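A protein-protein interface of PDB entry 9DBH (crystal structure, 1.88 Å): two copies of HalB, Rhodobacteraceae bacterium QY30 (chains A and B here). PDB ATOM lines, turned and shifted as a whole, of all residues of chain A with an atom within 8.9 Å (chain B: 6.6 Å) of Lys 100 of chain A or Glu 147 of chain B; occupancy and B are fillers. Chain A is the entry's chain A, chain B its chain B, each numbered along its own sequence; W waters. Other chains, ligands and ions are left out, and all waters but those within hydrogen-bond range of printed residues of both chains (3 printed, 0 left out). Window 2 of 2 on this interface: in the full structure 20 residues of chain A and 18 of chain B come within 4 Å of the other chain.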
ATOM      1  N   ASP A  67     -36.766  26.311   9.550  1.00  0.00           N
ATOM      2  CA  ASP A  67     -36.641  27.756   9.413  1.00  0.00           C
ATOM      3  C   ASP A  67     -35.879  28.393  10.565  1.00  0.00           C
ATOM      4  O   ASP A  67     -35.623  29.600  10.524  1.00  0.00           O
ATOM      5  CB  ASP A  67     -38.027  28.397   9.308  1.00  0.00           C
ATOM      6  CG  ASP A  67     -38.720  28.080   7.996  1.00  0.00           C
ATOM      7  OD1 ASP A  67     -38.056  27.526   7.097  1.00  0.00           O
ATOM      8  OD2 ASP A  67     -39.925  28.386   7.863  1.00  0.00           O
ATOM      9  N   GLY A  68     -35.528  27.627  11.593  1.00  0.00           N
ATOM     10  CA  GLY A  68     -34.823  28.196  12.721  1.00  0.00           C
ATOM     11  C   GLY A  68     -35.636  29.131  13.585  1.00  0.00           C
ATOM     12  O   GLY A  68     -35.059  30.014  14.229  1.00  0.00           O
ATOM     13  N   ILE A  73     -36.545  26.681  18.735  1.00  0.00           N
ATOM     14  CA  ILE A  73     -35.357  26.497  19.560  1.00  0.00           C
ATOM     15  C   ILE A  73     -35.761  26.294  21.016  1.00  0.00           C
ATOM     16  O   ILE A  73     -35.193  25.453  21.724  1.00  0.00           O
ATOM     17  CB  ILE A  73     -34.405  27.700  19.389  1.00  0.00           C
ATOM     18  CG1 ILE A  73     -33.959  27.810  17.924  1.00  0.00           C
ATOM     19  CG2 ILE A  73     -33.190  27.561  20.294  1.00  0.00           C
ATOM     20  CD1 ILE A  73     -33.082  29.032  17.633  1.00  0.00           C
ATOM     21  N   VAL A  97     -32.269  24.006  12.443  1.00  0.00           N
ATOM     22  CA  VAL A  97     -31.095  24.747  11.995  1.00  0.00           C
ATOM     23  C   VAL A  97     -31.119  26.078  12.727  1.00  0.00           C
ATOM     24  O   VAL A  97     -31.970  26.928  12.444  1.00  0.00           O
ATOM     25  CB  VAL A  97     -31.063  24.960  10.475  1.00  0.00           C
ATOM     26  CG1 VAL A  97     -29.772  25.697  10.067  1.00  0.00           C
ATOM     27  CG2 VAL A  97     -31.177  23.631   9.744  1.00  0.00           C
ATOM     28  N   ILE A  98     -30.216  26.244  13.688  1.00  0.00           N
ATOM     29  CA  ILE A  98     -30.116  27.492  14.435  1.00  0.00           C
ATOM     30  C   ILE A  98     -29.348  28.492  13.581  1.00  0.00           C
ATOM     31  O   ILE A  98     -28.199  28.244  13.204  1.00  0.00           O
ATOM     32  CB  ILE A  98     -29.423  27.273  15.787  1.00  0.00           C
ATOM     33  CG1 ILE A  98     -30.197  26.255  16.631  1.00  0.00           C
ATOM     34  CG2 ILE A  98     -29.274  28.606  16.525  1.00  0.00           C
ATOM     35  CD1 ILE A  98     -29.380  25.674  17.760  1.00  0.00           C
ATOM     36  N   ARG A  99     -29.978  29.620  13.277  1.00  0.00           N
ATOM     37  CA  ARG A  99     -29.353  30.574  12.379  1.00  0.00           C
ATOM     38  C   ARG A  99     -28.331  31.430  13.120  1.00  0.00           C
ATOM     39  O   ARG A  99     -28.307  31.500  14.353  1.00  0.00           O
ATOM     40  CB  ARG A  99     -30.406  31.453  11.709  1.00  0.00           C
ATOM     41  CG  ARG A  99     -31.264  30.691  10.719  1.00  0.00           C
ATOM     42  CD  ARG A  99     -32.166  31.597   9.903  1.00  0.00           C
ATOM     43  NE  ARG A  99     -33.504  31.666  10.464  1.00  0.00           N
ATOM     44  CZ  ARG A  99     -34.102  32.780  10.857  1.00  0.00           C
ATOM     45  NH1 ARG A  99     -33.520  33.963  10.730  1.00  0.00           N
ATOM     46  NH2 ARG A  99     -35.321  32.706  11.378  1.00  0.00           N
ATOM     47  N   LYS A 100     -27.460  32.067  12.329  1.00  0.00           N
ATOM     48  CA  LYS A 100     -26.474  33.022  12.814  1.00  0.00           C
ATOM     49  C   LYS A 100     -26.995  34.445  12.818  1.00  0.00           C
ATOM     50  O   LYS A 100     -26.455  35.291  13.539  1.00  0.00           O
ATOM     51  CB  LYS A 100     -25.225  32.995  11.923  1.00  0.00           C
ATOM     52  CG  LYS A 100     -24.728  31.612  11.595  1.00  0.00           C
ATOM     53  CD  LYS A 100     -23.832  31.087  12.697  1.00  0.00           C
ATOM     54  CE  LYS A 100     -23.315  29.700  12.372  1.00  0.00           C
ATOM     55  NZ  LYS A 100     -23.214  28.891  13.617  1.00  0.00           N
ATOM     56  N   ASP A 101     -28.023  34.715  12.020  1.00  0.00           N
ATOM     57  CA  ASP A 101     -28.507  36.064  11.751  1.00  0.00           C
ATOM     58  C   ASP A 101     -30.017  36.051  11.946  1.00  0.00           C
ATOM     59  O   ASP A 101     -30.749  35.506  11.109  1.00  0.00           O
ATOM     60  CB  ASP A 101     -28.135  36.489  10.327  1.00  0.00           C
ATOM     61  CG  ASP A 101     -28.484  37.938  10.019  1.00  0.00           C
ATOM     62  OD1 ASP A 101     -29.470  38.474  10.562  1.00  0.00           O
ATOM     63  OD2 ASP A 101     -27.760  38.546   9.203  1.00  0.00           O
ATOM     64  N   TYR A 102     -30.486  36.634  13.047  1.00  0.00           N
ATOM     65  CA  TYR A 102     -31.915  36.797  13.277  1.00  0.00           C
ATOM     66  C   TYR A 102     -32.370  38.227  13.028  1.00  0.00           C
ATOM     67  O   TYR A 102     -33.265  38.728  13.719  1.00  0.00           O
ATOM     68  CB  TYR A 102     -32.278  36.325  14.683  1.00  0.00           C
ATOM     69  CG  TYR A 102     -32.353  34.818  14.714  1.00  0.00           C
ATOM     70  CD1 TYR A 102     -33.528  34.164  14.381  1.00  0.00           C
ATOM     71  CD2 TYR A 102     -31.231  34.056  14.997  1.00  0.00           C
ATOM     72  CE1 TYR A 102     -33.593  32.785  14.365  1.00  0.00           C
ATOM     73  CE2 TYR A 102     -31.283  32.678  14.986  1.00  0.00           C
ATOM     74  CZ  TYR A 102     -32.463  32.047  14.667  1.00  0.00           C
ATOM     75  OH  TYR A 102     -32.504  30.676  14.656  1.00  0.00           O
ATOM     76  N   GLY A 103     -31.775  38.880  12.023  1.00  0.00           N
ATOM     77  CA  GLY A 103     -32.095  40.270  11.746  1.00  0.00           C
ATOM     78  C   GLY A 103     -33.524  40.469  11.279  1.00  0.00           C
ATOM     79  O   GLY A 103     -34.144  41.488  11.585  1.00  0.00           O
ATOM     80  N   GLU A 105     -36.229  38.695  12.243  1.00  0.00           N
ATOM     81  CA  GLU A 105     -37.074  38.633  13.430  1.00  0.00           C
ATOM     82  C   GLU A 105     -36.897  39.866  14.306  1.00  0.00           C
ATOM     83  O   GLU A 105     -37.877  40.408  14.838  1.00  0.00           O
ATOM     84  CB  GLU A 105     -36.755  37.365  14.221  1.00  0.00           C
ATOM     85  CG  GLU A 105     -37.262  36.073  13.582  1.00  0.00           C
ATOM     86  CD  GLU A 105     -36.422  35.587  12.410  1.00  0.00           C
ATOM     87  OE1 GLU A 105     -35.376  36.207  12.103  1.00  0.00           O
ATOM     88  OE2 GLU A 105     -36.812  34.570  11.799  1.00  0.00           O
ATOM     89  N   ILE A 106     -35.650  40.321  14.467  1.00  0.00           N
ATOM     90  CA  ILE A 106     -35.370  41.521  15.253  1.00  0.00           C
ATOM     91  C   ILE A 106     -36.076  42.725  14.650  1.00  0.00           C
ATOM     92  O   ILE A 106     -36.667  43.542  15.366  1.00  0.00           O
ATOM     93  CB  ILE A 106     -33.848  41.738  15.350  1.00  0.00           C
ATOM     94  CG1 ILE A 106     -33.230  40.732  16.321  1.00  0.00           C
ATOM     95  CG2 ILE A 106     -33.510  43.183  15.751  1.00  0.00           C
ATOM     96  CD1 ILE A 106     -31.715  40.712  16.299  1.00  0.00           C
ATOM     97  N   ALA A 143     -33.437  36.779  20.211  1.00  0.00           N
ATOM     98  CA  ALA A 143     -32.688  36.719  18.960  1.00  0.00           C
ATOM     99  C   ALA A 143     -31.244  37.167  19.161  1.00  0.00           C
ATOM    100  O   ALA A 143     -30.308  36.522  18.670  1.00  0.00           O
ATOM    101  CB  ALA A 143     -33.372  37.581  17.902  1.00  0.00           C
ATOM    102  N   ARG A 144     -31.043  38.286  19.864  1.00  0.00           N
ATOM    103  CA  ARG A 144     -29.682  38.772  20.087  1.00  0.00           C
ATOM    104  C   ARG A 144     -28.858  37.753  20.861  1.00  0.00           C
ATOM    105  O   ARG A 144     -27.676  37.540  20.564  1.00  0.00           O
ATOM    106  CB  ARG A 144     -29.704  40.109  20.831  1.00  0.00           C
ATOM    107  CG  ARG A 144     -30.084  41.296  19.966  1.00  0.00           C
ATOM    108  CD  ARG A 144     -29.162  41.417  18.761  1.00  0.00           C
ATOM    109  NE  ARG A 144     -29.311  42.714  18.111  1.00  0.00           N
ATOM    110  CZ  ARG A 144     -28.914  42.997  16.878  1.00  0.00           C
ATOM    111  NH1 ARG A 144     -28.337  42.086  16.110  1.00  0.00           N
ATOM    112  NH2 ARG A 144     -29.108  44.223  16.403  1.00  0.00           N
ATOM    113  N   LEU A 145     -29.470  37.094  21.843  1.00  0.00           N
ATOM    114  CA  LEU A 145     -28.726  36.126  22.639  1.00  0.00           C
ATOM    115  C   LEU A 145     -28.421  34.868  21.836  1.00  0.00           C
ATOM    116  O   LEU A 145     -27.317  34.318  21.935  1.00  0.00           O
ATOM    117  CB  LEU A 145     -29.497  35.805  23.917  1.00  0.00           C
ATOM    118  CG  LEU A 145     -29.485  36.998  24.876  1.00  0.00           C
ATOM    119  CD1 LEU A 145     -30.425  36.801  26.055  1.00  0.00           C
ATOM    120  CD2 LEU A 145     -28.064  37.266  25.356  1.00  0.00           C
ATOM    121  N   VAL A 146     -29.374  34.408  21.018  1.00  0.00           N
ATOM    122  CA  VAL A 146     -29.100  33.278  20.132  1.00  0.00           C
ATOM    123  C   VAL A 146     -27.962  33.619  19.180  1.00  0.00           C
ATOM    124  O   VAL A 146     -27.077  32.790  18.926  1.00  0.00           O
ATOM    125  CB  VAL A 146     -30.368  32.864  19.363  1.00  0.00           C
ATOM    126  CG1 VAL A 146     -30.021  31.843  18.275  1.00  0.00           C
ATOM    127  CG2 VAL A 146     -31.400  32.279  20.311  1.00  0.00           C
ATOM    128  N   GLU A 147     -27.960  34.844  18.642  1.00  0.00           N
ATOM    129  CA  GLU A 147     -26.887  35.266  17.743  1.00  0.00           C
ATOM    130  C   GLU A 147     -25.518  35.153  18.403  1.00  0.00           C
ATOM    131  O   GLU A 147     -24.514  34.915  17.718  1.00  0.00           O
ATOM    132  CB  GLU A 147     -27.131  36.704  17.263  1.00  0.00           C
ATOM    133  CG  GLU A 147     -28.173  36.814  16.150  1.00  0.00           C
ATOM    134  CD  GLU A 147     -28.442  38.247  15.717  1.00  0.00           C
ATOM    135  OE1 GLU A 147     -28.046  39.181  16.446  1.00  0.00           O
ATOM    136  OE2 GLU A 147     -29.057  38.436  14.645  1.00  0.00           O
ATOM    137  N   SER A 148     -25.456  35.296  19.723  1.00  0.00           N
ATOM    138  CA  SER A 148     -24.203  35.212  20.460  1.00  0.00           C
ATOM    139  C   SER A 148     -23.871  33.798  20.920  1.00  0.00           C
ATOM    140  O   SER A 148     -22.854  33.601  21.595  1.00  0.00           O
ATOM    141  CB  SER A 148     -24.246  36.143  21.676  1.00  0.00           C
ATOM    142  OG  SER A 148     -25.082  35.611  22.692  1.00  0.00           O
ATOM    143  N   GLY A 149     -24.698  32.812  20.585  1.00  0.00           N
ATOM    144  CA  GLY A 149     -24.445  31.439  20.964  1.00  0.00           C
ATOM    145  C   GLY A 149     -25.158  30.979  22.220  1.00  0.00           C
ATOM    146  O   GLY A 149     -25.023  29.806  22.593  1.00  0.00           O
ATOM    147  N   LEU B  70     -19.112  19.746  22.901  1.00  0.00           N
ATOM    148  CA  LEU B  70     -20.074  19.075  22.029  1.00  0.00           C
ATOM    149  C   LEU B  70     -20.975  18.124  22.817  1.00  0.00           C
ATOM    150  O   LEU B  70     -22.184  18.050  22.564  1.00  0.00           O
ATOM    151  CB  LEU B  70     -19.335  18.328  20.918  1.00  0.00           C
ATOM    152  CG  LEU B  70     -18.662  19.212  19.862  1.00  0.00           C
ATOM    153  CD1 LEU B  70     -17.985  18.349  18.814  1.00  0.00           C
ATOM    154  CD2 LEU B  70     -19.697  20.139  19.226  1.00  0.00           C
ATOM    155  N   ILE B  98     -22.790  27.948  22.774  1.00  0.00           N
ATOM    156  CA  ILE B  98     -22.344  27.242  21.583  1.00  0.00           C
ATOM    157  C   ILE B  98     -21.234  28.058  20.932  1.00  0.00           C
ATOM    158  O   ILE B  98     -21.431  29.223  20.575  1.00  0.00           O
ATOM    159  CB  ILE B  98     -23.523  27.000  20.631  1.00  0.00           C
ATOM    160  CG1 ILE B  98     -24.599  26.195  21.359  1.00  0.00           C
ATOM    161  CG2 ILE B  98     -23.071  26.274  19.366  1.00  0.00           C
ATOM    162  CD1 ILE B  98     -25.910  26.054  20.609  1.00  0.00           C
ATOM    163  N   ARG B  99     -20.049  27.464  20.817  1.00  0.00           N
ATOM    164  CA  ARG B  99     -18.910  28.173  20.259  1.00  0.00           C
ATOM    165  C   ARG B  99     -19.157  28.499  18.787  1.00  0.00           C
ATOM    166  O   ARG B  99     -19.921  27.829  18.091  1.00  0.00           O
ATOM    167  CB  ARG B  99     -17.625  27.350  20.407  1.00  0.00           C
ATOM    168  CG  ARG B  99     -17.252  27.007  21.853  1.00  0.00           C
ATOM    169  CD  ARG B  99     -16.247  25.859  21.944  1.00  0.00           C
ATOM    170  NE  ARG B  99     -14.864  26.309  21.869  1.00  0.00           N
ATOM    171  CZ  ARG B  99     -14.135  26.674  22.916  1.00  0.00           C
ATOM    172  NH1 ARG B  99     -14.644  26.709  24.136  1.00  0.00           N
ATOM    173  NH2 ARG B  99     -12.859  27.003  22.736  1.00  0.00           N
ATOM    174  N   LYS B 100     -18.498  29.551  18.308  1.00  0.00           N
ATOM    175  CA  LYS B 100     -18.644  29.897  16.901  1.00  0.00           C
ATOM    176  C   LYS B 100     -17.806  29.008  15.994  1.00  0.00           C
ATOM    177  O   LYS B 100     -18.098  28.913  14.798  1.00  0.00           O
ATOM    178  CB  LYS B 100     -18.294  31.367  16.687  1.00  0.00           C
ATOM    179  CG  LYS B 100     -19.357  32.315  17.224  1.00  0.00           C
ATOM    180  CD  LYS B 100     -20.500  32.498  16.230  1.00  0.00           C
ATOM    181  CE  LYS B 100     -21.871  32.275  16.868  1.00  0.00           C
ATOM    182  NZ  LYS B 100     -22.101  33.049  18.126  1.00  0.00           N
ATOM    183  N   ASP B 101     -16.805  28.326  16.544  1.00  0.00           N
ATOM    184  CA  ASP B 101     -15.905  27.488  15.769  1.00  0.00           C
ATOM    185  C   ASP B 101     -15.562  26.258  16.598  1.00  0.00           C
ATOM    186  O   ASP B 101     -15.332  26.359  17.808  1.00  0.00           O
ATOM    187  CB  ASP B 101     -14.646  28.277  15.363  1.00  0.00           C
ATOM    188  CG  ASP B 101     -13.456  27.387  15.054  1.00  0.00           C
ATOM    189  OD1 ASP B 101     -13.318  26.921  13.902  1.00  0.00           O
ATOM    190  OD2 ASP B 101     -12.643  27.164  15.971  1.00  0.00           O
ATOM    191  N   TYR B 102     -15.584  25.090  15.956  1.00  0.00           N
ATOM    192  CA  TYR B 102     -15.170  23.845  16.586  1.00  0.00           C
ATOM    193  C   TYR B 102     -13.962  23.250  15.863  1.00  0.00           C
ATOM    194  O   TYR B 102     -13.787  22.032  15.823  1.00  0.00           O
ATOM    195  CB  TYR B 102     -16.338  22.858  16.655  1.00  0.00           C
ATOM    196  CG  TYR B 102     -17.300  23.233  17.768  1.00  0.00           C
ATOM    197  CD1 TYR B 102     -17.114  22.752  19.056  1.00  0.00           C
ATOM    198  CD2 TYR B 102     -18.343  24.114  17.537  1.00  0.00           C
ATOM    199  CE1 TYR B 102     -17.958  23.114  20.078  1.00  0.00           C
ATOM    200  CE2 TYR B 102     -19.193  24.484  18.552  1.00  0.00           C
ATOM    201  CZ  TYR B 102     -18.994  23.978  19.818  1.00  0.00           C
ATOM    202  OH  TYR B 102     -19.823  24.340  20.838  1.00  0.00           O
ATOM    203  N   GLY B 103     -13.112  24.119  15.303  1.00  0.00           N
ATOM    204  CA  GLY B 103     -11.944  23.645  14.575  1.00  0.00           C
ATOM    205  C   GLY B 103     -10.978  22.877  15.454  1.00  0.00           C
ATOM    206  O   GLY B 103     -10.353  21.912  15.011  1.00  0.00           O
ATOM    207  N   ARG B 104     -10.853  23.283  16.717  1.00  0.00           N
ATOM    208  CA  ARG B 104      -9.989  22.558  17.642  1.00  0.00           C
ATOM    209  C   ARG B 104     -10.445  21.110  17.792  1.00  0.00           C
ATOM    210  O   ARG B 104      -9.632  20.179  17.728  1.00  0.00           O
ATOM    211  CB  ARG B 104      -9.981  23.265  18.993  1.00  0.00           C
ATOM    212  CG  ARG B 104      -9.062  22.648  20.024  1.00  0.00           C
ATOM    213  CD  ARG B 104      -9.183  23.386  21.341  1.00  0.00           C
ATOM    214  NE  ARG B 104     -10.562  23.430  21.821  1.00  0.00           N
ATOM    215  CZ  ARG B 104     -10.931  23.936  22.990  1.00  0.00           C
ATOM    216  NH1 ARG B 104     -10.045  24.441  23.833  1.00  0.00           N
ATOM    217  NH2 ARG B 104     -12.218  23.933  23.321  1.00  0.00           N
ATOM    218  N   ILE B 106     -12.397  19.407  15.709  1.00  0.00           N
ATOM    219  CA  ILE B 106     -12.246  18.745  14.415  1.00  0.00           C
ATOM    220  C   ILE B 106     -10.804  18.285  14.204  1.00  0.00           C
ATOM    221  O   ILE B 106     -10.559  17.177  13.709  1.00  0.00           O
ATOM    222  CB  ILE B 106     -12.707  19.694  13.293  1.00  0.00           C
ATOM    223  CG1 ILE B 106     -14.222  19.892  13.360  1.00  0.00           C
ATOM    224  CG2 ILE B 106     -12.284  19.186  11.922  1.00  0.00           C
ATOM    225  CD1 ILE B 106     -14.702  21.165  12.689  1.00  0.00           C
ATOM    226  N   ILE B 142     -20.237  15.623  14.060  1.00  0.00           N
ATOM    227  CA  ILE B 142     -20.983  16.450  15.008  1.00  0.00           C
ATOM    228  C   ILE B 142     -20.471  17.889  14.986  1.00  0.00           C
ATOM    229  O   ILE B 142     -21.254  18.845  14.922  1.00  0.00           O
ATOM    230  CB  ILE B 142     -20.892  15.859  16.425  1.00  0.00           C
ATOM    231  CG1 ILE B 142     -21.593  14.502  16.507  1.00  0.00           C
ATOM    232  CG2 ILE B 142     -21.471  16.830  17.444  1.00  0.00           C
ATOM    233  CD1 ILE B 142     -21.237  13.747  17.763  1.00  0.00           C
ATOM    234  N   ALA B 143     -19.148  18.064  15.058  1.00  0.00           N
ATOM    235  CA  ALA B 143     -18.580  19.408  15.130  1.00  0.00           C
ATOM    236  C   ALA B 143     -18.935  20.227  13.896  1.00  0.00           C
ATOM    237  O   ALA B 143     -19.331  21.393  13.999  1.00  0.00           O
ATOM    238  CB  ALA B 143     -17.061  19.321  15.305  1.00  0.00           C
ATOM    239  N   ARG B 144     -18.801  19.632  12.712  1.00  0.00           N
ATOM    240  CA  ARG B 144     -19.087  20.389  11.501  1.00  0.00           C
ATOM    241  C   ARG B 144     -20.579  20.657  11.346  1.00  0.00           C
ATOM    242  O   ARG B 144     -20.969  21.701  10.808  1.00  0.00           O
ATOM    243  CB  ARG B 144     -18.519  19.654  10.287  1.00  0.00           C
ATOM    244  CG  ARG B 144     -16.991  19.672  10.272  1.00  0.00           C
ATOM    245  CD  ARG B 144     -16.417  19.193   8.964  1.00  0.00           C
ATOM    246  NE  ARG B 144     -16.905  19.976   7.834  1.00  0.00           N
ATOM    247  CZ  ARG B 144     -16.487  19.811   6.588  1.00  0.00           C
ATOM    248  NH1 ARG B 144     -15.545  18.930   6.290  1.00  0.00           N
ATOM    249  NH2 ARG B 144     -17.028  20.542   5.619  1.00  0.00           N
ATOM    250  N   LEU B 145     -21.428  19.755  11.837  1.00  0.00           N
ATOM    251  CA  LEU B 145     -22.862  20.016  11.782  1.00  0.00           C
ATOM    252  C   LEU B 145     -23.268  21.065  12.811  1.00  0.00           C
ATOM    253  O   LEU B 145     -24.120  21.915  12.530  1.00  0.00           O
ATOM    254  CB  LEU B 145     -23.635  18.714  11.970  1.00  0.00           C
ATOM    255  CG  LEU B 145     -23.503  17.796  10.751  1.00  0.00           C
ATOM    256  CD1 LEU B 145     -24.016  16.399  11.053  1.00  0.00           C
ATOM    257  CD2 LEU B 145     -24.245  18.393   9.563  1.00  0.00           C
ATOM    258  N   VAL B 146     -22.652  21.042  13.995  1.00  0.00           N
ATOM    259  CA  VAL B 146     -22.932  22.071  14.995  1.00  0.00           C
ATOM    260  C   VAL B 146     -22.504  23.441  14.480  1.00  0.00           C
ATOM    261  O   VAL B 146     -23.229  24.435  14.635  1.00  0.00           O
ATOM    262  CB  VAL B 146     -22.254  21.728  16.338  1.00  0.00           C
ATOM    263  CG1 VAL B 146     -22.203  22.954  17.247  1.00  0.00           C
ATOM    264  CG2 VAL B 146     -23.009  20.595  17.044  1.00  0.00           C
ATOM    265  N   GLU B 147     -21.333  23.517  13.839  1.00  0.00           N
ATOM    266  CA  GLU B 147     -20.906  24.784  13.245  1.00  0.00           C
ATOM    267  C   GLU B 147     -21.922  25.312  12.242  1.00  0.00           C
ATOM    268  O   GLU B 147     -22.051  26.530  12.071  1.00  0.00           O
ATOM    269  CB  GLU B 147     -19.546  24.615  12.562  1.00  0.00           C
ATOM    270  CG  GLU B 147     -18.375  24.437  13.510  1.00  0.00           C
ATOM    271  CD  GLU B 147     -17.039  24.400  12.772  1.00  0.00           C
ATOM    272  OE1 GLU B 147     -17.020  24.068  11.567  1.00  0.00           O
ATOM    273  OE2 GLU B 147     -16.005  24.708  13.397  1.00  0.00           O
ATOM    274  N   SER B 148     -22.648  24.423  11.570  1.00  0.00           N
ATOM    275  CA  SER B 148     -23.642  24.831  10.589  1.00  0.00           C
ATOM    276  C   SER B 148     -25.008  25.106  11.206  1.00  0.00           C
ATOM    277  O   SER B 148     -25.953  25.409  10.470  1.00  0.00           O
ATOM    278  CB  SER B 148     -23.777  23.766   9.494  1.00  0.00           C
ATOM    279  OG  SER B 148     -24.496  22.637   9.964  1.00  0.00           O
ATOM    280  N   GLY B 149     -25.136  25.007  12.527  1.00  0.00           N
ATOM    281  CA  GLY B 149     -26.374  25.316  13.215  1.00  0.00           C
ATOM    282  C   GLY B 149     -27.265  24.136  13.540  1.00  0.00           C
ATOM    283  O   GLY B 149     -28.423  24.346  13.919  1.00  0.00           O
ATOM    284  N   LYS B 150     -26.771  22.912  13.414  1.00  0.00           N
ATOM    285  CA  LYS B 150     -27.588  21.730  13.644  1.00  0.00           C
ATOM    286  C   LYS B 150     -27.281  21.116  15.008  1.00  0.00           C
ATOM    287  O   LYS B 150     -26.308  21.469  15.675  1.00  0.00           O
ATOM    288  CB  LYS B 150     -27.381  20.717  12.513  1.00  0.00           C
ATOM    289  CG  LYS B 150     -27.727  21.291  11.141  1.00  0.00           C
ATOM    290  CD  LYS B 150     -28.202  20.229  10.155  1.00  0.00           C
ATOM    291  CE  LYS B 150     -29.412  19.460  10.681  1.00  0.00           C
ATOM    292  NZ  LYS B 150     -30.708  20.212  10.633  1.00  0.00           N
HETATM  293  O   HOH W   1     -22.588  27.161  15.630  1.00  0.00           O
HETATM  294  O   HOH W   2     -20.371  32.001  20.999  1.00  0.00           O
HETATM  295  O   HOH W   3     -26.768  28.242  10.696  1.00  0.00           O
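Ile 98 of chain A touches Gly 149 of chain B, and with the chains exchanged Gly 149 of chain A touches Ile 98 of chain B. Lys 100 of chain A touches Glu 147 of chain B, and with the chains exchanged Glu 147 of chain A touches Lys 100 of chain B. Ser 148 of chain A touches Lys 100 of chain B, but with the chains exchanged Lys 100 of chain A does not touch Ser 148 of chain B (4.8 Å). Gly 149 of chain A touches Lys 100 of chain B, but with the chains exchanged Lys 100 of chain A does not touch Gly 149 of chain B (4.5 Å). Positions printed for both chains: 98, 99, 100, 101, 102, 103, 106, 143, 144, 145, 146, 147, 148 and 149. Of the 9 pairs that touch across the chains among the printed residues, 4 have their exchanged pair printed and touching as well.
The backbone NH (N) of Ile 98 of chain A sits at hydrogen-bond distance from the backbone carbonyl oxygen (O) of Gly 149 of chain B. NZ of Lys 100 of chain A is in hydrogen-bond range of O of Glu 147 of chain B. The side-chain amino group (NZ) of Lys 100 of chain B is in hydrogen-bond range of the backbone carbonyl oxygen (O) of Glu 147 of chain A, 3.1 Å away. The backbone NH (N) of Ile 98 of chain B sits at hydrogen-bond distance from the backbone carbonyl oxygen (O) of Gly 149 of chain A (2.9 Å).
Water W1 bridges the side-chain amino group (NZ) of Lys 100 of chain A (2.7 Å) and the backbone carbonyl oxygen (O) of Val 146 of chain B (3.0 Å). Water W3 lies within hydrogen-bond range of the backbone carbonyl oxygen (O) of Ile 98 of chain A and the backbone carbonyl oxygen (O) of Ser 148 of chain B. Water W2 lies within hydrogen-bond range of the backbone carbonyl oxygen of Ile 98 of chain B (3.0 Å) and the backbone carbonyl oxygen of Ser 148 of chain A (3.0 Å).
Of the 18 printed residues of chain B, 6 touch a printed residue of chain A. Hydrophobic or aromatic side chains of chain B that line the printed part of chain A: Ile 98. Of the 19 printed residues of chain A, 6 touch a printed residue of chain B. Among the printed residues, no Asp or Glu carboxylate lies within 4 Å of a Lys or Arg side-chain nitrogen of the other chain.
Among the printed residues, pairs that only touch across the chains: Val 97 of chain A with Ser 148 of chain B (3.9 Å), Val 97 of chain A with Gly 149 of chain B (3.3 Å), Val 97 of chain A with Lys 150 of chain B (3.6 Å), Ser 148 of chain A with Lys 100 of chain B (3.4 Å) and Gly 149 of chain A with Lys 100 of chain B (3.6 Å).
N of Tyr 102 of chain A lies within hydrogen-bond range of OE2 of Glu 147 of chain A (2.8 Å). OE1 of Glu 147 of chain A is in salt-bridge range of NH1 of Arg 144 of chain A (2.9 Å). O of Leu 145 of chain A sits at hydrogen-bond distance from OG of Ser 148 of chain A, 2.7 Å away. The backbone NH (N) of Tyr 102 of chain B lies within hydrogen-bond range of the side-chain carboxylate (OE2) of Glu 147 of chain B (2.6 Å). O of Leu 145 of chain B sits at hydrogen-bond distance from OG of Ser 148 of chain B, at 2.7 Å. N of Lys 150 of chain B lies within hydrogen-bond range of O of Leu 145 of chain B, 3.0 Å away.
Of chain B, only Glu 147 comes within 4 Å of Lys 100 of chain A. Asp 101 of chain A touches none of the printed residues of chain B. Of the printed residues of chain B, Ser 148 of chain A touches Lys 100 (3.4 Å). Printed residues of chain B within 4 Å of Gly 149 of chain A: Ile 98 (2.9 Å) and Lys 100 (3.6 Å). Of the printed residues of chain A, Lys 100 of chain B touches Glu 147 (3.1 Å), Ser 148 (3.4 Å) and Gly 149 (3.6 Å). Asp 101 of chain B touches none of the printed residues of chain A. Of chain A, only Lys 100 comes within 4 Å of Glu 147 of chain B. Ser 148 of chain B touches one residue of chain A. The nearest residue of chain B that does not touch Lys 100 of chain A is Gly 149 of chain B (4.5 Å).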
